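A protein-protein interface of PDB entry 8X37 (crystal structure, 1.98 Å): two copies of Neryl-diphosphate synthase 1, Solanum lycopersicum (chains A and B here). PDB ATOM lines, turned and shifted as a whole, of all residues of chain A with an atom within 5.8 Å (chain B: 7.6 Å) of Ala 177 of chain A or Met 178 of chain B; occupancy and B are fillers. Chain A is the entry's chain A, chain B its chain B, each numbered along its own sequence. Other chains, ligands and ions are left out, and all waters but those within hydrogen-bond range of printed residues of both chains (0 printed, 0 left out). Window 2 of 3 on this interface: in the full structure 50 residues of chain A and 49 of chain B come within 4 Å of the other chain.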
ATOM      1  N   SER A 172     -17.635  20.012   5.449  1.00  0.00           N
ATOM      2  CA  SER A 172     -18.371  19.664   4.251  1.00  0.00           C
ATOM      3  C   SER A 172     -17.774  20.394   3.043  1.00  0.00           C
ATOM      4  O   SER A 172     -17.624  19.804   1.980  1.00  0.00           O
ATOM      5  CB  SER A 172     -19.853  19.897   4.449  1.00  0.00           C
ATOM      6  OG  SER A 172     -20.553  20.031   3.216  1.00  0.00           O
ATOM      7  N   ILE A 173     -17.402  21.671   3.194  1.00  0.00           N
ATOM      8  CA  ILE A 173     -16.814  22.431   2.093  1.00  0.00           C
ATOM      9  C   ILE A 173     -15.428  21.879   1.722  1.00  0.00           C
ATOM     10  O   ILE A 173     -15.020  21.915   0.558  1.00  0.00           O
ATOM     11  CB  ILE A 173     -16.756  23.933   2.443  1.00  0.00           C
ATOM     12  CG1 ILE A 173     -18.144  24.542   2.449  1.00  0.00           C
ATOM     13  CG2 ILE A 173     -15.848  24.694   1.473  1.00  0.00           C
ATOM     14  CD1 ILE A 173     -18.216  25.910   3.104  1.00  0.00           C
ATOM     15  N   VAL A 174     -14.670  21.438   2.725  1.00  0.00           N
ATOM     16  CA  VAL A 174     -13.345  20.892   2.491  1.00  0.00           C
ATOM     17  C   VAL A 174     -13.472  19.601   1.666  1.00  0.00           C
ATOM     18  O   VAL A 174     -12.728  19.403   0.709  1.00  0.00           O
ATOM     19  CB  VAL A 174     -12.603  20.656   3.821  1.00  0.00           C
ATOM     20  CG1 VAL A 174     -11.411  19.732   3.630  1.00  0.00           C
ATOM     21  CG2 VAL A 174     -12.163  21.953   4.485  1.00  0.00           C
ATOM     22  N   ASN A 175     -14.420  18.728   2.042  1.00  0.00           N
ATOM     23  CA  ASN A 175     -14.700  17.499   1.309  1.00  0.00           C
ATOM     24  C   ASN A 175     -14.994  17.798  -0.157  1.00  0.00           C
ATOM     25  O   ASN A 175     -14.471  17.121  -1.028  1.00  0.00           O
ATOM     26  CB  ASN A 175     -15.870  16.727   1.909  1.00  0.00           C
ATOM     27  CG  ASN A 175     -15.435  15.628   2.849  1.00  0.00           C
ATOM     28  OD1 ASN A 175     -14.968  15.888   3.960  1.00  0.00           O
ATOM     29  ND2 ASN A 175     -15.611  14.382   2.433  1.00  0.00           N
ATOM     30  N   LYS A 176     -15.835  18.803  -0.427  1.00  0.00           N
ATOM     31  CA  LYS A 176     -16.194  19.159  -1.793  1.00  0.00           C
ATOM     32  C   LYS A 176     -14.967  19.627  -2.583  1.00  0.00           C
ATOM     33  O   LYS A 176     -14.818  19.302  -3.772  1.00  0.00           O
ATOM     34  CB  LYS A 176     -17.295  20.224  -1.793  1.00  0.00           C
ATOM     35  CG  LYS A 176     -18.706  19.738  -1.486  1.00  0.00           C
ATOM     36  CD  LYS A 176     -18.816  18.659  -0.409  1.00  0.00           C
ATOM     37  CE  LYS A 176     -20.219  18.227  -0.141  1.00  0.00           C
ATOM     38  NZ  LYS A 176     -21.094  19.356   0.200  1.00  0.00           N
ATOM     39  N   ALA A 177     -14.087  20.401  -1.932  1.00  0.00           N
ATOM     40  CA  ALA A 177     -12.912  20.907  -2.621  1.00  0.00           C
ATOM     41  C   ALA A 177     -11.960  19.753  -2.949  1.00  0.00           C
ATOM     42  O   ALA A 177     -11.304  19.771  -3.984  1.00  0.00           O
ATOM     43  CB  ALA A 177     -12.235  21.961  -1.790  1.00  0.00           C
ATOM     44  N   MET A 178     -11.894  18.754  -2.062  1.00  0.00           N
ATOM     45  CA  MET A 178     -11.030  17.605  -2.263  1.00  0.00           C
ATOM     46  C   MET A 178     -11.519  16.761  -3.443  1.00  0.00           C
ATOM     47  O   MET A 178     -10.709  16.151  -4.134  1.00  0.00           O
ATOM     48  CB  MET A 178     -10.990  16.698  -1.033  1.00  0.00           C
ATOM     49  CG  MET A 178     -10.684  17.419   0.251  1.00  0.00           C
ATOM     50  SD  MET A 178      -9.036  17.129   0.896  1.00  0.00           S
ATOM     51  CE  MET A 178      -9.509  16.238   2.389  1.00  0.00           C
ATOM     52  N   ASN A 179     -12.833  16.738  -3.687  1.00  0.00           N
ATOM     53  CA  ASN A 179     -13.427  15.909  -4.726  1.00  0.00           C
ATOM     54  C   ASN A 179     -13.659  16.692  -6.019  1.00  0.00           C
ATOM     55  O   ASN A 179     -14.449  16.268  -6.860  1.00  0.00           O
ATOM     56  CB  ASN A 179     -14.754  15.315  -4.278  1.00  0.00           C
ATOM     57  CG  ASN A 179     -14.586  14.350  -3.134  1.00  0.00           C
ATOM     58  OD1 ASN A 179     -13.546  14.333  -2.464  1.00  0.00           O
ATOM     59  ND2 ASN A 179     -15.604  13.550  -2.881  1.00  0.00           N
ATOM     60  N   GLY A 180     -12.981  17.838  -6.161  1.00  0.00           N
ATOM     61  CA  GLY A 180     -12.957  18.584  -7.407  1.00  0.00           C
ATOM     62  C   GLY A 180     -14.272  19.294  -7.709  1.00  0.00           C
ATOM     63  O   GLY A 180     -14.489  19.682  -8.852  1.00  0.00           O
ATOM     64  N   LEU A 181     -15.129  19.496  -6.700  1.00  0.00           N
ATOM     65  CA  LEU A 181     -16.438  20.104  -6.927  1.00  0.00           C
ATOM     66  C   LEU A 181     -16.340  21.628  -6.896  1.00  0.00           C
ATOM     67  O   LEU A 181     -17.222  22.293  -7.443  1.00  0.00           O
ATOM     68  CB  LEU A 181     -17.478  19.606  -5.923  1.00  0.00           C
ATOM     69  CG  LEU A 181     -18.255  18.339  -6.302  1.00  0.00           C
ATOM     70  CD1 LEU A 181     -17.410  17.324  -7.051  1.00  0.00           C
ATOM     71  CD2 LEU A 181     -18.831  17.687  -5.058  1.00  0.00           C
ATOM     72  N   LEU A 182     -15.292  22.175  -6.261  1.00  0.00           N
ATOM     73  CA  LEU A 182     -15.203  23.617  -6.135  1.00  0.00           C
ATOM     74  C   LEU A 182     -13.767  24.058  -5.901  1.00  0.00           C
ATOM     75  O   LEU A 182     -12.927  23.278  -5.461  1.00  0.00           O
ATOM     76  CB  LEU A 182     -16.135  24.107  -5.024  1.00  0.00           C
ATOM     77  CG  LEU A 182     -15.858  23.597  -3.604  1.00  0.00           C
ATOM     78  CD1 LEU A 182     -14.841  24.443  -2.861  1.00  0.00           C
ATOM     79  CD2 LEU A 182     -17.164  23.562  -2.837  1.00  0.00           C
ATOM     80  N   ASP A 183     -13.539  25.342  -6.206  1.00  0.00           N
ATOM     81  CA  ASP A 183     -12.275  26.031  -6.015  1.00  0.00           C
ATOM     82  C   ASP A 183     -12.427  27.034  -4.868  1.00  0.00           C
ATOM     83  O   ASP A 183     -13.528  27.468  -4.551  1.00  0.00           O
ATOM     84  CB  ASP A 183     -11.878  26.856  -7.235  1.00  0.00           C
ATOM     85  CG  ASP A 183     -11.984  26.219  -8.619  1.00  0.00           C
ATOM     86  OD1 ASP A 183     -11.349  25.166  -8.830  1.00  0.00           O
ATOM     87  OD2 ASP A 183     -12.670  26.797  -9.501  1.00  0.00           O
ATOM     88  N   LYS B 171     -11.203  29.400   3.661  1.00  0.00           N
ATOM     89  CA  LYS B 171     -10.331  29.282   2.499  1.00  0.00           C
ATOM     90  C   LYS B 171      -8.915  28.817   2.875  1.00  0.00           C
ATOM     91  O   LYS B 171      -8.318  27.992   2.183  1.00  0.00           O
ATOM     92  CB  LYS B 171     -10.215  30.630   1.789  1.00  0.00           C
ATOM     93  CG  LYS B 171     -11.509  31.123   1.195  1.00  0.00           C
ATOM     94  CD  LYS B 171     -11.311  32.373   0.347  1.00  0.00           C
ATOM     95  CE  LYS B 171     -12.642  33.003   0.059  1.00  0.00           C
ATOM     96  NZ  LYS B 171     -12.521  34.305  -0.602  1.00  0.00           N
ATOM     97  N   SER B 172      -8.357  29.380   3.946  1.00  0.00           N
ATOM     98  CA  SER B 172      -7.025  29.022   4.395  1.00  0.00           C
ATOM     99  C   SER B 172      -6.977  27.534   4.769  1.00  0.00           C
ATOM    100  O   SER B 172      -6.042  26.822   4.398  1.00  0.00           O
ATOM    101  CB  SER B 172      -6.586  29.950   5.511  1.00  0.00           C
ATOM    102  OG  SER B 172      -5.548  29.402   6.316  1.00  0.00           O
ATOM    103  N   ILE B 173      -8.005  27.047   5.478  1.00  0.00           N
ATOM    104  CA  ILE B 173      -8.082  25.652   5.890  1.00  0.00           C
ATOM    105  C   ILE B 173      -8.223  24.725   4.680  1.00  0.00           C
ATOM    106  O   ILE B 173      -7.691  23.611   4.682  1.00  0.00           O
ATOM    107  CB  ILE B 173      -9.226  25.486   6.904  1.00  0.00           C
ATOM    108  CG1 ILE B 173      -8.828  26.086   8.242  1.00  0.00           C
ATOM    109  CG2 ILE B 173      -9.670  24.031   7.038  1.00  0.00           C
ATOM    110  CD1 ILE B 173      -9.975  26.274   9.224  1.00  0.00           C
ATOM    111  N   VAL B 174      -8.984  25.168   3.673  1.00  0.00           N
ATOM    112  CA  VAL B 174      -9.230  24.380   2.484  1.00  0.00           C
ATOM    113  C   VAL B 174      -7.910  24.201   1.740  1.00  0.00           C
ATOM    114  O   VAL B 174      -7.616  23.091   1.293  1.00  0.00           O
ATOM    115  CB  VAL B 174     -10.308  25.042   1.592  1.00  0.00           C
ATOM    116  CG1 VAL B 174     -10.229  24.607   0.139  1.00  0.00           C
ATOM    117  CG2 VAL B 174     -11.716  24.823   2.141  1.00  0.00           C
ATOM    118  N   ASN B 175      -7.145  25.296   1.594  1.00  0.00           N
ATOM    119  CA  ASN B 175      -5.877  25.264   0.891  1.00  0.00           C
ATOM    120  C   ASN B 175      -4.937  24.264   1.550  1.00  0.00           C
ATOM    121  O   ASN B 175      -4.311  23.476   0.859  1.00  0.00           O
ATOM    122  CB  ASN B 175      -5.225  26.635   0.810  1.00  0.00           C
ATOM    123  CG  ASN B 175      -5.764  27.419  -0.363  1.00  0.00           C
ATOM    124  OD1 ASN B 175      -6.190  26.836  -1.368  1.00  0.00           O
ATOM    125  ND2 ASN B 175      -5.768  28.739  -0.264  1.00  0.00           N
ATOM    126  N   LYS B 176      -4.859  24.294   2.884  1.00  0.00           N
ATOM    127  CA  LYS B 176      -4.024  23.361   3.622  1.00  0.00           C
ATOM    128  C   LYS B 176      -4.463  21.914   3.395  1.00  0.00           C
ATOM    129  O   LYS B 176      -3.618  21.044   3.271  1.00  0.00           O
ATOM    130  CB  LYS B 176      -4.006  23.737   5.104  1.00  0.00           C
ATOM    131  CG  LYS B 176      -3.094  24.941   5.351  1.00  0.00           C
ATOM    132  CD  LYS B 176      -3.132  25.507   6.758  1.00  0.00           C
ATOM    133  CE  LYS B 176      -2.616  26.910   6.764  1.00  0.00           C
ATOM    134  NZ  LYS B 176      -2.455  27.339   8.152  1.00  0.00           N
ATOM    135  N   ALA B 177      -5.768  21.642   3.386  1.00  0.00           N
ATOM    136  CA  ALA B 177      -6.238  20.272   3.220  1.00  0.00           C
ATOM    137  C   ALA B 177      -5.911  19.780   1.811  1.00  0.00           C
ATOM    138  O   ALA B 177      -5.625  18.608   1.610  1.00  0.00           O
ATOM    139  CB  ALA B 177      -7.729  20.183   3.488  1.00  0.00           C
ATOM    140  N   MET B 178      -5.965  20.686   0.832  1.00  0.00           N
ATOM    141  CA  MET B 178      -5.677  20.325  -0.542  1.00  0.00           C
ATOM    142  C   MET B 178      -4.193  19.986  -0.725  1.00  0.00           C
ATOM    143  O   MET B 178      -3.848  19.214  -1.613  1.00  0.00           O
ATOM    144  CB  MET B 178      -6.038  21.477  -1.475  1.00  0.00           C
ATOM    145  CG  MET B 178      -7.513  21.791  -1.504  1.00  0.00           C
ATOM    146  SD  MET B 178      -8.422  20.707  -2.618  1.00  0.00           S
ATOM    147  CE  MET B 178      -9.033  22.008  -3.710  1.00  0.00           C
ATOM    148  N   ASN B 179      -3.321  20.578   0.093  1.00  0.00           N
ATOM    149  CA  ASN B 179      -1.884  20.396  -0.025  1.00  0.00           C
ATOM    150  C   ASN B 179      -1.352  19.395   1.000  1.00  0.00           C
ATOM    151  O   ASN B 179      -0.148  19.376   1.259  1.00  0.00           O
ATOM    152  CB  ASN B 179      -1.145  21.714   0.171  1.00  0.00           C
ATOM    153  CG  ASN B 179      -1.409  22.674  -0.960  1.00  0.00           C
ATOM    154  OD1 ASN B 179      -1.661  22.245  -2.090  1.00  0.00           O
ATOM    155  ND2 ASN B 179      -1.323  23.965  -0.684  1.00  0.00           N
ATOM    156  N   GLY B 180      -2.231  18.588   1.600  1.00  0.00           N
ATOM    157  CA  GLY B 180      -1.800  17.496   2.463  1.00  0.00           C
ATOM    158  C   GLY B 180      -1.253  17.954   3.814  1.00  0.00           C
ATOM    159  O   GLY B 180      -0.655  17.161   4.531  1.00  0.00           O
ATOM    160  N   LEU B 181      -1.511  19.211   4.206  1.00  0.00           N
ATOM    161  CA  LEU B 181      -0.964  19.762   5.439  1.00  0.00           C
ATOM    162  C   LEU B 181      -1.890  19.501   6.625  1.00  0.00           C
ATOM    163  O   LEU B 181      -1.472  19.647   7.764  1.00  0.00           O
ATOM    164  CB  LEU B 181      -0.680  21.245   5.249  1.00  0.00           C
ATOM    165  CG  LEU B 181       0.317  21.582   4.136  1.00  0.00           C
ATOM    166  CD1 LEU B 181       0.670  23.066   4.124  1.00  0.00           C
ATOM    167  CD2 LEU B 181       1.595  20.741   4.245  1.00  0.00           C
ATOM    168  N   LEU B 182      -3.145  19.118   6.366  1.00  0.00           N
ATOM    169  CA  LEU B 182      -4.061  18.687   7.414  1.00  0.00           C
ATOM    170  C   LEU B 182      -5.155  17.833   6.782  1.00  0.00           C
ATOM    171  O   LEU B 182      -5.317  17.862   5.568  1.00  0.00           O
ATOM    172  CB  LEU B 182      -4.635  19.896   8.151  1.00  0.00           C
ATOM    173  CG  LEU B 182      -5.474  20.890   7.338  1.00  0.00           C
ATOM    174  CD1 LEU B 182      -6.942  20.486   7.153  1.00  0.00           C
ATOM    175  CD2 LEU B 182      -5.410  22.245   8.014  1.00  0.00           C
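Val 174 of chain A touches its own counterpart, Val 174 of chain B. Val 174 of chain A touches Ala 177 of chain B, and with the chains exchanged Ala 177 of chain A touches Val 174 of chain B. Ala 177 of chain A touches Met 178 of chain B, and with the chains exchanged Met 178 of chain A touches Ala 177 of chain B. Positions printed for both chains: 172, 173, 174, 175, 176, 177, 178, 179, 180, 181 and 182. Of the 5 pairs that touch across the chains among the printed residues, 5 have their exchanged pair printed and touching as well.
The side-chain sulfur (SD) of Met 178 of chain B sits close to the backbone carbonyl oxygen (O) of Ala 177 of chain A, at 3.3 Å. The side-chain sulfur (SD) of Met 178 of chain A lies close to the backbone carbonyl oxygen (O) of Ala 177 of chain B (3.8 Å).
Val 174 of chain B touches Val 174 of chain A (CG2 to CG2, 3.7 Å). CG1 of Val 174 of chain A touches CB of Ala 177 of chain B, at 3.7 Å. Val 174 of chain B touches Ala 177 of chain A.
Printed residues of chain A that touch a printed residue of chain B: Val 174, Ala 177 and Met 178. Hydrophobic or aromatic side chains of chain A that line the printed part of chain B: Val 174, Ala 177 and Met 178. Along chain A the printed residues that touch a printed residue of chain B span positions 174 to 178. Printed residues of chain B that touch a printed residue of chain A: Val 174, Ala 177 and Met 178. Hydrophobic or aromatic side chains of chain B within 4 Å of the printed part of chain A: Val 174, Ala 177 and Met 178. Along chain B the printed residues that touch a printed residue of chain A span positions 174 to 178. Among the printed residues, no Asp or Glu carboxylate lies within 4 Å of a Lys or Arg side-chain nitrogen of the other chain.
Ala 177 of chain A touches two residues of chain B. Of chain A, only Ala 177 comes within 4 Å of Met 178 of chain B. Of the printed residues of chain A, Ala 177 of chain B touches Val 174 (3.7 Å) and Met 178 (3.8 Å). Printed residues of chain B within 4 Å of Met 178 of chain A: Ala 177 (3.8 Å). Of the printed residues of chain A, Val 174 of chain B touches Val 174 (3.7 Å) and Ala 177 (3.8 Å). Printed residues of chain B within 4 Å of Val 174 of chain A: Val 174 and Ala 177. Lys 171 of chain B touches none of the printed residues of chain A. The nearest residue of chain B that does not touch Ala 177 of chain A is Asn 175 of chain B (7.0 Å). The nearest residue of chain A that does not touch Met 178 of chain B is Met 178 of chain A (4.02 Å).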
